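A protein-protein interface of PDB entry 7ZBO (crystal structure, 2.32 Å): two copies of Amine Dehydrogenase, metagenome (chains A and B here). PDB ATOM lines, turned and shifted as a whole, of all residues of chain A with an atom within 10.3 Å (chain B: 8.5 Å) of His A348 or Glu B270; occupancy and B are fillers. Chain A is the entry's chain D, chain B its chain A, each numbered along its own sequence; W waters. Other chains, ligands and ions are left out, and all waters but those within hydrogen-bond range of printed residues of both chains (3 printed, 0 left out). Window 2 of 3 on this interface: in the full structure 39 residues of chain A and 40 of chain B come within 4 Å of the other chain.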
ATOM      1  N   ARG A  31      -0.267  17.354  34.722  1.00  0.00           N
ATOM      2  CA  ARG A  31       1.169  17.494  35.101  1.00  0.00           C
ATOM      3  C   ARG A  31       1.477  16.582  36.293  1.00  0.00           C
ATOM      4  O   ARG A  31       0.974  16.838  37.354  1.00  0.00           O
ATOM      5  CB  ARG A  31       1.505  18.947  35.438  1.00  0.00           C
ATOM      6  CG  ARG A  31       1.788  19.840  34.238  1.00  0.00           C
ATOM      7  CD  ARG A  31       3.116  19.512  33.602  1.00  0.00           C
ATOM      8  NE  ARG A  31       4.241  20.030  34.350  1.00  0.00           N
ATOM      9  CZ  ARG A  31       4.892  21.161  34.083  1.00  0.00           C
ATOM     10  NH1 ARG A  31       4.524  21.930  33.059  1.00  0.00           N
ATOM     11  NH2 ARG A  31       5.942  21.487  34.835  1.00  0.00           N
ATOM     12  N   LYS A  32       2.312  15.566  36.108  1.00  0.00           N
ATOM     13  CA  LYS A  32       2.619  14.533  37.138  1.00  0.00           C
ATOM     14  C   LYS A  32       3.644  15.071  38.148  1.00  0.00           C
ATOM     15  O   LYS A  32       3.810  14.412  39.179  1.00  0.00           O
ATOM     16  CB  LYS A  32       3.072  13.236  36.453  1.00  0.00           C
ATOM     17  N   ASP A  33       4.261  16.242  37.923  1.00  0.00           N
ATOM     18  CA  ASP A  33       5.185  16.902  38.896  1.00  0.00           C
ATOM     19  C   ASP A  33       4.425  17.866  39.828  1.00  0.00           C
ATOM     20  O   ASP A  33       5.072  18.524  40.668  1.00  0.00           O
ATOM     21  CB  ASP A  33       6.342  17.615  38.190  1.00  0.00           C
ATOM     22  CG  ASP A  33       5.967  18.660  37.141  1.00  0.00           C
ATOM     23  OD1 ASP A  33       4.782  18.687  36.697  1.00  0.00           O
ATOM     24  OD2 ASP A  33       6.889  19.418  36.735  1.00  0.00           O
ATOM     25  N   GLU A 344      10.714  28.405  31.989  1.00  0.00           N
ATOM     26  CA  GLU A 344      11.207  27.003  31.978  1.00  0.00           C
ATOM     27  C   GLU A 344      10.869  26.324  30.635  1.00  0.00           C
ATOM     28  O   GLU A 344       9.683  26.337  30.235  1.00  0.00           O
ATOM     29  CB  GLU A 344      10.610  26.223  33.144  1.00  0.00           C
ATOM     30  CG  GLU A 344      11.334  24.926  33.458  1.00  0.00           C
ATOM     31  CD  GLU A 344      12.831  25.057  33.699  1.00  0.00           C
ATOM     32  OE1 GLU A 344      13.592  24.321  33.037  1.00  0.00           O
ATOM     33  OE2 GLU A 344      13.245  25.907  34.521  1.00  0.00           O
ATOM     34  N   ALA A 345      11.888  25.750  29.969  1.00  0.00           N
ATOM     35  CA  ALA A 345      11.824  25.168  28.601  1.00  0.00           C
ATOM     36  C   ALA A 345      10.804  24.025  28.526  1.00  0.00           C
ATOM     37  O   ALA A 345      10.644  23.293  29.517  1.00  0.00           O
ATOM     38  CB  ALA A 345      13.182  24.681  28.178  1.00  0.00           C
ATOM     39  N   TYR A 346      10.116  23.903  27.385  1.00  0.00           N
ATOM     40  CA  TYR A 346       9.249  22.744  27.070  1.00  0.00           C
ATOM     41  C   TYR A 346      10.126  21.497  27.018  1.00  0.00           C
ATOM     42  O   TYR A 346      11.205  21.539  26.449  1.00  0.00           O
ATOM     43  CB  TYR A 346       8.504  22.859  25.738  1.00  0.00           C
ATOM     44  CG  TYR A 346       7.675  21.631  25.453  1.00  0.00           C
ATOM     45  CD1 TYR A 346       6.459  21.439  26.080  1.00  0.00           C
ATOM     46  CD2 TYR A 346       8.125  20.621  24.628  1.00  0.00           C
ATOM     47  CE1 TYR A 346       5.694  20.303  25.862  1.00  0.00           C
ATOM     48  CE2 TYR A 346       7.371  19.475  24.401  1.00  0.00           C
ATOM     49  CZ  TYR A 346       6.144  19.319  25.011  1.00  0.00           C
ATOM     50  OH  TYR A 346       5.394  18.200  24.809  1.00  0.00           O
ATOM     51  N   VAL A 347       9.658  20.411  27.596  1.00  0.00           N
ATOM     52  CA  VAL A 347      10.364  19.107  27.526  1.00  0.00           C
ATOM     53  C   VAL A 347       9.261  18.052  27.526  1.00  0.00           C
ATOM     54  O   VAL A 347       8.264  18.254  28.223  1.00  0.00           O
ATOM     55  CB  VAL A 347      11.382  18.977  28.687  1.00  0.00           C
ATOM     56  CG1 VAL A 347      10.812  18.284  29.916  1.00  0.00           C
ATOM     57  CG2 VAL A 347      12.666  18.300  28.239  1.00  0.00           C
ATOM     58  N   HIS A 348       9.390  16.998  26.726  1.00  0.00           N
ATOM     59  CA  HIS A 348       8.495  15.818  26.783  1.00  0.00           C
ATOM     60  C   HIS A 348       8.735  15.075  28.109  1.00  0.00           C
ATOM     61  O   HIS A 348       9.822  15.171  28.674  1.00  0.00           O
ATOM     62  CB  HIS A 348       8.706  14.924  25.564  1.00  0.00           C
ATOM     63  CG  HIS A 348       7.981  13.627  25.677  1.00  0.00           C
ATOM     64  ND1 HIS A 348       6.718  13.447  25.146  1.00  0.00           N
ATOM     65  CD2 HIS A 348       8.324  12.481  26.331  1.00  0.00           C
ATOM     66  CE1 HIS A 348       6.308  12.219  25.448  1.00  0.00           C
ATOM     67  NE2 HIS A 348       7.286  11.604  26.178  1.00  0.00           N
ATOM     68  N   GLY A 349       7.711  14.389  28.594  1.00  0.00           N
ATOM     69  CA  GLY A 349       7.787  13.434  29.715  1.00  0.00           C
ATOM     70  C   GLY A 349       7.187  13.955  30.995  1.00  0.00           C
ATOM     71  O   GLY A 349       7.316  13.195  31.984  1.00  0.00           O
ATOM     72  N   ARG A 350       6.551  15.135  30.992  1.00  0.00           N
ATOM     73  CA  ARG A 350       5.991  15.775  32.216  1.00  0.00           C
ATOM     74  C   ARG A 350       4.532  15.350  32.390  1.00  0.00           C
ATOM     75  O   ARG A 350       4.032  15.545  33.496  1.00  0.00           O
ATOM     76  CB  ARG A 350       6.098  17.308  32.164  1.00  0.00           C
ATOM     77  CG  ARG A 350       7.533  17.814  32.164  1.00  0.00           C
ATOM     78  CD  ARG A 350       7.677  19.319  32.284  1.00  0.00           C
ATOM     79  NE  ARG A 350       7.032  20.098  31.215  1.00  0.00           N
ATOM     80  CZ  ARG A 350       7.520  21.220  30.690  1.00  0.00           C
ATOM     81  NH1 ARG A 350       8.684  21.680  31.117  1.00  0.00           N
ATOM     82  NH2 ARG A 350       6.891  21.836  29.697  1.00  0.00           N
ATOM     83  N   LEU A 351       3.894  14.785  31.345  1.00  0.00           N
ATOM     84  CA  LEU A 351       2.447  14.411  31.322  1.00  0.00           C
ATOM     85  C   LEU A 351       2.260  12.883  31.309  1.00  0.00           C
ATOM     86  O   LEU A 351       3.104  12.123  31.794  1.00  0.00           O
ATOM     87  CB  LEU A 351       1.761  15.048  30.106  1.00  0.00           C
ATOM     88  CG  LEU A 351       2.079  16.517  29.848  1.00  0.00           C
ATOM     89  CD1 LEU A 351       1.184  17.038  28.737  1.00  0.00           C
ATOM     90  CD2 LEU A 351       1.906  17.366  31.100  1.00  0.00           C
ATOM     91  N   HIS B 160       2.016  23.449  26.515  1.00  0.00           N
ATOM     92  CA  HIS B 160       1.659  22.360  27.465  1.00  0.00           C
ATOM     93  C   HIS B 160       2.009  21.011  26.819  1.00  0.00           C
ATOM     94  O   HIS B 160       2.578  20.112  27.499  1.00  0.00           O
ATOM     95  CB  HIS B 160       0.178  22.491  27.835  1.00  0.00           C
ATOM     96  CG  HIS B 160      -0.346  21.377  28.663  1.00  0.00           C
ATOM     97  ND1 HIS B 160       0.077  21.161  29.967  1.00  0.00           N
ATOM     98  CD2 HIS B 160      -1.265  20.421  28.392  1.00  0.00           C
ATOM     99  CE1 HIS B 160      -0.546  20.106  30.446  1.00  0.00           C
ATOM    100  NE2 HIS B 160      -1.359  19.623  29.501  1.00  0.00           N
ATOM    101  N   LYS B 161       1.645  20.884  25.539  1.00  0.00           N
ATOM    102  CA  LYS B 161       1.909  19.699  24.688  1.00  0.00           C
ATOM    103  C   LYS B 161       2.288  20.178  23.286  1.00  0.00           C
ATOM    104  O   LYS B 161       1.535  21.029  22.726  1.00  0.00           O
ATOM    105  CB  LYS B 161       0.661  18.814  24.649  1.00  0.00           C
ATOM    106  CG  LYS B 161       0.857  17.460  23.979  1.00  0.00           C
ATOM    107  CD  LYS B 161      -0.357  16.543  24.123  1.00  0.00           C
ATOM    108  CE  LYS B 161      -0.043  15.057  24.075  1.00  0.00           C
ATOM    109  NZ  LYS B 161      -0.967  14.315  24.965  1.00  0.00           N
ATOM    110  N   ILE B 162       3.406  19.688  22.741  1.00  0.00           N
ATOM    111  CA  ILE B 162       3.789  19.964  21.321  1.00  0.00           C
ATOM    112  C   ILE B 162       3.510  18.699  20.497  1.00  0.00           C
ATOM    113  O   ILE B 162       4.129  17.671  20.813  1.00  0.00           O
ATOM    114  CB  ILE B 162       5.256  20.415  21.185  1.00  0.00           C
ATOM    115  CG1 ILE B 162       5.580  21.597  22.107  1.00  0.00           C
ATOM    116  CG2 ILE B 162       5.579  20.701  19.712  1.00  0.00           C
ATOM    117  CD1 ILE B 162       6.940  22.261  21.844  1.00  0.00           C
ATOM    118  N   ASP B 163       2.632  18.775  19.483  1.00  0.00           N
ATOM    119  CA  ASP B 163       2.400  17.688  18.497  1.00  0.00           C
ATOM    120  C   ASP B 163       3.285  17.908  17.266  1.00  0.00           C
ATOM    121  O   ASP B 163       3.720  16.904  16.672  1.00  0.00           O
ATOM    122  CB  ASP B 163       0.933  17.606  18.101  1.00  0.00           C
ATOM    123  CG  ASP B 163       0.020  17.221  19.250  1.00  0.00           C
ATOM    124  OD1 ASP B 163       0.442  16.377  20.107  1.00  0.00           O
ATOM    125  OD2 ASP B 163      -1.108  17.799  19.303  1.00  0.00           O
ATOM    126  N   PHE B 219      16.062  20.747  17.938  1.00  0.00           N
ATOM    127  CA  PHE B 219      14.711  20.763  18.554  1.00  0.00           C
ATOM    128  C   PHE B 219      14.469  19.408  19.220  1.00  0.00           C
ATOM    129  O   PHE B 219      14.069  19.393  20.391  1.00  0.00           O
ATOM    130  CB  PHE B 219      13.640  21.158  17.535  1.00  0.00           C
ATOM    131  CG  PHE B 219      13.625  22.633  17.207  1.00  0.00           C
ATOM    132  CD1 PHE B 219      13.553  23.590  18.205  1.00  0.00           C
ATOM    133  CD2 PHE B 219      13.738  23.076  15.910  1.00  0.00           C
ATOM    134  CE1 PHE B 219      13.558  24.942  17.909  1.00  0.00           C
ATOM    135  CE2 PHE B 219      13.766  24.429  15.609  1.00  0.00           C
ATOM    136  CZ  PHE B 219      13.657  25.360  16.606  1.00  0.00           C
ATOM    137  N   ALA B 220      14.740  18.304  18.538  1.00  0.00           N
ATOM    138  CA  ALA B 220      14.497  16.959  19.091  1.00  0.00           C
ATOM    139  C   ALA B 220      15.295  16.809  20.385  1.00  0.00           C
ATOM    140  O   ALA B 220      14.767  16.213  21.333  1.00  0.00           O
ATOM    141  CB  ALA B 220      14.880  15.907  18.094  1.00  0.00           C
ATOM    142  N   SER B 221      16.509  17.346  20.438  1.00  0.00           N
ATOM    143  CA  SER B 221      17.349  17.308  21.663  1.00  0.00           C
ATOM    144  C   SER B 221      16.718  18.206  22.751  1.00  0.00           C
ATOM    145  O   SER B 221      16.530  17.716  23.872  1.00  0.00           O
ATOM    146  CB  SER B 221      18.780  17.701  21.382  1.00  0.00           C
ATOM    147  OG  SER B 221      19.501  17.904  22.589  1.00  0.00           O
ATOM    148  N   ALA B 222      16.361  19.452  22.414  1.00  0.00           N
ATOM    149  CA  ALA B 222      15.801  20.452  23.350  1.00  0.00           C
ATOM    150  C   ALA B 222      14.509  19.922  23.996  1.00  0.00           C
ATOM    151  O   ALA B 222      14.370  20.047  25.227  1.00  0.00           O
ATOM    152  CB  ALA B 222      15.558  21.744  22.621  1.00  0.00           C
ATOM    153  N   PHE B 223      13.600  19.353  23.194  1.00  0.00           N
ATOM    154  CA  PHE B 223      12.260  18.884  23.618  1.00  0.00           C
ATOM    155  C   PHE B 223      12.345  17.489  24.254  1.00  0.00           C
ATOM    156  O   PHE B 223      11.285  16.970  24.651  1.00  0.00           O
ATOM    157  CB  PHE B 223      11.288  18.896  22.441  1.00  0.00           C
ATOM    158  CG  PHE B 223      11.064  20.238  21.789  1.00  0.00           C
ATOM    159  CD1 PHE B 223      11.402  21.417  22.432  1.00  0.00           C
ATOM    160  CD2 PHE B 223      10.458  20.328  20.545  1.00  0.00           C
ATOM    161  CE1 PHE B 223      11.209  22.643  21.810  1.00  0.00           C
ATOM    162  CE2 PHE B 223      10.238  21.552  19.940  1.00  0.00           C
ATOM    163  CZ  PHE B 223      10.604  22.708  20.578  1.00  0.00           C
ATOM    164  N   GLY B 224      13.539  16.892  24.365  1.00  0.00           N
ATOM    165  CA  GLY B 224      13.718  15.561  24.987  1.00  0.00           C
ATOM    166  C   GLY B 224      12.984  14.478  24.216  1.00  0.00           C
ATOM    167  O   GLY B 224      12.297  13.666  24.850  1.00  0.00           O
ATOM    168  N   LEU B 225      13.078  14.505  22.881  1.00  0.00           N
ATOM    169  CA  LEU B 225      12.422  13.541  21.963  1.00  0.00           C
ATOM    170  C   LEU B 225      13.475  12.534  21.471  1.00  0.00           C
ATOM    171  O   LEU B 225      14.700  12.820  21.547  1.00  0.00           O
ATOM    172  CB  LEU B 225      11.790  14.302  20.790  1.00  0.00           C
ATOM    173  CG  LEU B 225      10.675  15.284  21.157  1.00  0.00           C
ATOM    174  CD1 LEU B 225      10.271  16.119  19.953  1.00  0.00           C
ATOM    175  CD2 LEU B 225       9.454  14.579  21.748  1.00  0.00           C
ATOM    176  N   THR B 226      13.009  11.395  20.966  1.00  0.00           N
ATOM    177  CA  THR B 226      13.855  10.302  20.431  1.00  0.00           C
ATOM    178  C   THR B 226      13.578  10.209  18.929  1.00  0.00           C
ATOM    179  O   THR B 226      12.430   9.829  18.542  1.00  0.00           O
ATOM    180  CB  THR B 226      13.596   8.990  21.183  1.00  0.00           C
ATOM    181  OG1 THR B 226      13.398   9.308  22.555  1.00  0.00           O
ATOM    182  CG2 THR B 226      14.743   8.011  21.047  1.00  0.00           C
ATOM    183  N   VAL B 227      14.581  10.566  18.120  1.00  0.00           N
ATOM    184  CA  VAL B 227      14.466  10.594  16.632  1.00  0.00           C
ATOM    185  C   VAL B 227      14.342   9.154  16.100  1.00  0.00           C
ATOM    186  O   VAL B 227      15.163   8.308  16.478  1.00  0.00           O
ATOM    187  CB  VAL B 227      15.669  11.334  16.017  1.00  0.00           C
ATOM    188  CG1 VAL B 227      15.690  11.233  14.494  1.00  0.00           C
ATOM    189  CG2 VAL B 227      15.688  12.791  16.497  1.00  0.00           C
ATOM    190  N   ILE B 228      13.340   8.894  15.260  1.00  0.00           N
ATOM    191  CA  ILE B 228      13.255   7.666  14.418  1.00  0.00           C
ATOM    192  C   ILE B 228      14.089   7.928  13.150  1.00  0.00           C
ATOM    193  O   ILE B 228      15.170   7.336  13.015  1.00  0.00           O
ATOM    194  CB  ILE B 228      11.780   7.299  14.123  1.00  0.00           C
ATOM    195  CG1 ILE B 228      11.069   6.816  15.382  1.00  0.00           C
ATOM    196  CG2 ILE B 228      11.698   6.264  13.004  1.00  0.00           C
ATOM    197  CD1 ILE B 228       9.555   6.700  15.259  1.00  0.00           C
ATOM    198  N   THR B 267      10.592  12.349  12.266  1.00  0.00           N
ATOM    199  CA  THR B 267       9.619  11.574  13.076  1.00  0.00           C
ATOM    200  C   THR B 267      10.327  11.103  14.348  1.00  0.00           C
ATOM    201  O   THR B 267      11.567  11.053  14.377  1.00  0.00           O
ATOM    202  CB  THR B 267       9.017  10.422  12.259  1.00  0.00           C
ATOM    203  OG1 THR B 267      10.095   9.691  11.670  1.00  0.00           O
ATOM    204  CG2 THR B 267       8.089  10.909  11.167  1.00  0.00           C
ATOM    205  N   THR B 268       9.547  10.749  15.355  1.00  0.00           N
ATOM    206  CA  THR B 268       9.978  10.702  16.768  1.00  0.00           C
ATOM    207  C   THR B 268       9.220   9.545  17.432  1.00  0.00           C
ATOM    208  O   THR B 268       8.076   9.260  16.998  1.00  0.00           O
ATOM    209  CB  THR B 268       9.771  12.119  17.323  1.00  0.00           C
ATOM    210  OG1 THR B 268      10.977  12.643  17.883  1.00  0.00           O
ATOM    211  CG2 THR B 268       8.637  12.195  18.304  1.00  0.00           C
ATOM    212  N   GLU B 269       9.810   8.888  18.424  1.00  0.00           N
ATOM    213  CA  GLU B 269       9.157   7.731  19.090  1.00  0.00           C
ATOM    214  C   GLU B 269       7.921   8.221  19.858  1.00  0.00           C
ATOM    215  O   GLU B 269       7.004   7.412  20.104  1.00  0.00           O
ATOM    216  CB  GLU B 269      10.132   6.998  20.020  1.00  0.00           C
ATOM    217  CG  GLU B 269      11.336   6.364  19.310  1.00  0.00           C
ATOM    218  CD  GLU B 269      11.721   4.924  19.649  1.00  0.00           C
ATOM    219  OE1 GLU B 269      11.039   4.015  19.084  1.00  0.00           O
ATOM    220  OE2 GLU B 269      12.709   4.707  20.439  1.00  0.00           O
ATOM    221  N   GLU B 270       7.874   9.518  20.172  1.00  0.00           N
ATOM    222  CA  GLU B 270       6.809  10.163  20.970  1.00  0.00           C
ATOM    223  C   GLU B 270       5.641  10.602  20.076  1.00  0.00           C
ATOM    224  O   GLU B 270       4.623  11.032  20.630  1.00  0.00           O
ATOM    225  CB  GLU B 270       7.396  11.339  21.759  1.00  0.00           C
ATOM    226  CG  GLU B 270       8.388  10.916  22.839  1.00  0.00           C
ATOM    227  CD  GLU B 270       9.820  10.653  22.401  1.00  0.00           C
ATOM    228  OE1 GLU B 270      10.170  10.967  21.231  1.00  0.00           O
ATOM    229  OE2 GLU B 270      10.591  10.138  23.223  1.00  0.00           O
ATOM    230  N   GLY B 271       5.754  10.507  18.754  1.00  0.00           N
ATOM    231  CA  GLY B 271       4.666  10.906  17.836  1.00  0.00           C
ATOM    232  C   GLY B 271       4.722  12.387  17.463  1.00  0.00           C
ATOM    233  O   GLY B 271       3.872  12.811  16.720  1.00  0.00           O
ATOM    234  N   VAL B 272       5.693  13.141  17.986  1.00  0.00           N
ATOM    235  CA  VAL B 272       5.926  14.578  17.655  1.00  0.00           C
ATOM    236  C   VAL B 272       6.563  14.663  16.269  1.00  0.00           C
ATOM    237  O   VAL B 272       7.577  13.981  16.057  1.00  0.00           O
ATOM    238  CB  VAL B 272       6.811  15.275  18.710  1.00  0.00           C
ATOM    239  CG1 VAL B 272       7.052  16.736  18.363  1.00  0.00           C
ATOM    240  CG2 VAL B 272       6.231  15.118  20.109  1.00  0.00           C
ATOM    241  N   ILE B 273       6.010  15.486  15.382  1.00  0.00           N
ATOM    242  CA  ILE B 273       6.574  15.739  14.024  1.00  0.00           C
ATOM    243  C   ILE B 273       7.297  17.081  14.037  1.00  0.00           C
ATOM    244  O   ILE B 273       6.760  18.015  14.616  1.00  0.00           O
ATOM    245  CB  ILE B 273       5.476  15.629  12.941  1.00  0.00           C
ATOM    246  CG1 ILE B 273       5.004  14.179  12.815  1.00  0.00           C
ATOM    247  CG2 ILE B 273       5.970  16.137  11.610  1.00  0.00           C
ATOM    248  CD1 ILE B 273       3.750  14.001  12.000  1.00  0.00           C
ATOM    249  N   ILE B 274       8.495  17.159  13.429  1.00  0.00           N
ATOM    250  CA  ILE B 274       9.285  18.417  13.280  1.00  0.00           C
ATOM    251  C   ILE B 274       9.568  18.625  11.790  1.00  0.00           C
ATOM    252  O   ILE B 274      10.280  17.794  11.211  1.00  0.00           O
ATOM    253  CB  ILE B 274      10.572  18.330  14.108  1.00  0.00           C
ATOM    254  CG1 ILE B 274      10.304  18.054  15.595  1.00  0.00           C
ATOM    255  CG2 ILE B 274      11.424  19.573  13.912  1.00  0.00           C
ATOM    256  CD1 ILE B 274      11.584  17.779  16.408  1.00  0.00           C
HETATM  257  O   HOH W   1      12.674  23.048  24.822  1.00  0.00           O
HETATM  258  O   HOH W   2       2.485  22.074  31.343  1.00  0.00           O
HETATM  259  O   HOH W   3       3.992  17.474  26.932  1.00  0.00           O
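His A348 touches just these residues of chain B: Phe B223, Gly B224, Leu B225 and Glu B270. Printed residues of chain A within 4 Å of Lys B161: Tyr A346. Of the printed residues of chain A, Ile B162 touches Tyr A346. Of chain A, only His A348 (3.9 Å) comes within 4 Å of Gly B224. Of chain A, only His A348 (3.9 Å) comes within 4 Å of Leu B225. No residue of chain A comes within 4 Å of Thr B268. Glu B270 touches one residue of chain A. No residue of chain A comes within 4 Å of Gly B271. Ile B273 touches none of the printed residues of chain A. The nearest residue of chain B that does not touch His A348 is Val B272 (5.3 Å).
No position is printed for both chains. Of the 11 pairs that touch across the chains among the printed residues, none has its exchanged pair printed and touching as well.
The backbone NH of Ile B162 is in hydrogen-bond range of the side-chain hydroxyl of Tyr A346, at 3.2 Å. The backbone carbonyl oxygen of Phe B223 sits at hydrogen-bond distance from the backbone NH of His A348 (2.8 Å).
O of His B160 touches CE1 of Tyr A346, 3.5 Å away. Lys B161 touches Tyr A346. O of Ala B222 touches O of Tyr A346, at 3.7 Å. O of Ala B222 touches CG2 of Val A347, 3.9 Å away. Phe B223 touches Val A347 (O to C, 3.7 Å). Gly B224 touches His A348. CB of His A348 touches CD2 of Leu B225, at 3.9 Å. Glu B270 touches His A348. CD1 of Leu A351 touches O of His B160 (3.6 Å).
The backbone carbonyl oxygen (O) of Ala B220 is in hydrogen-bond range of the backbone NH (N) of Leu B225 (2.9 Å). OE1 of Glu B270 is in hydrogen-bond range of N of Thr B226.
Of the 11 printed residues of chain A, 4 touch a printed residue of chain B. Hydrophobic or aromatic side chains of chain A that line the printed part of chain B: Tyr A346, Val A347, His A348 and Leu A351. Among the printed residues, 11 pairs touch across the chains.
Water W3 lies within hydrogen-bond range of the side-chain hydroxyl of Tyr A346 and the backbone carbonyl oxygen of His B160. Water W1 bridges O of Tyr A346 and O of Ala B222. Water W2 bridges NH1 of Arg A31 (2.7 Å) and ND1 of His B160 (2.9 Å).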
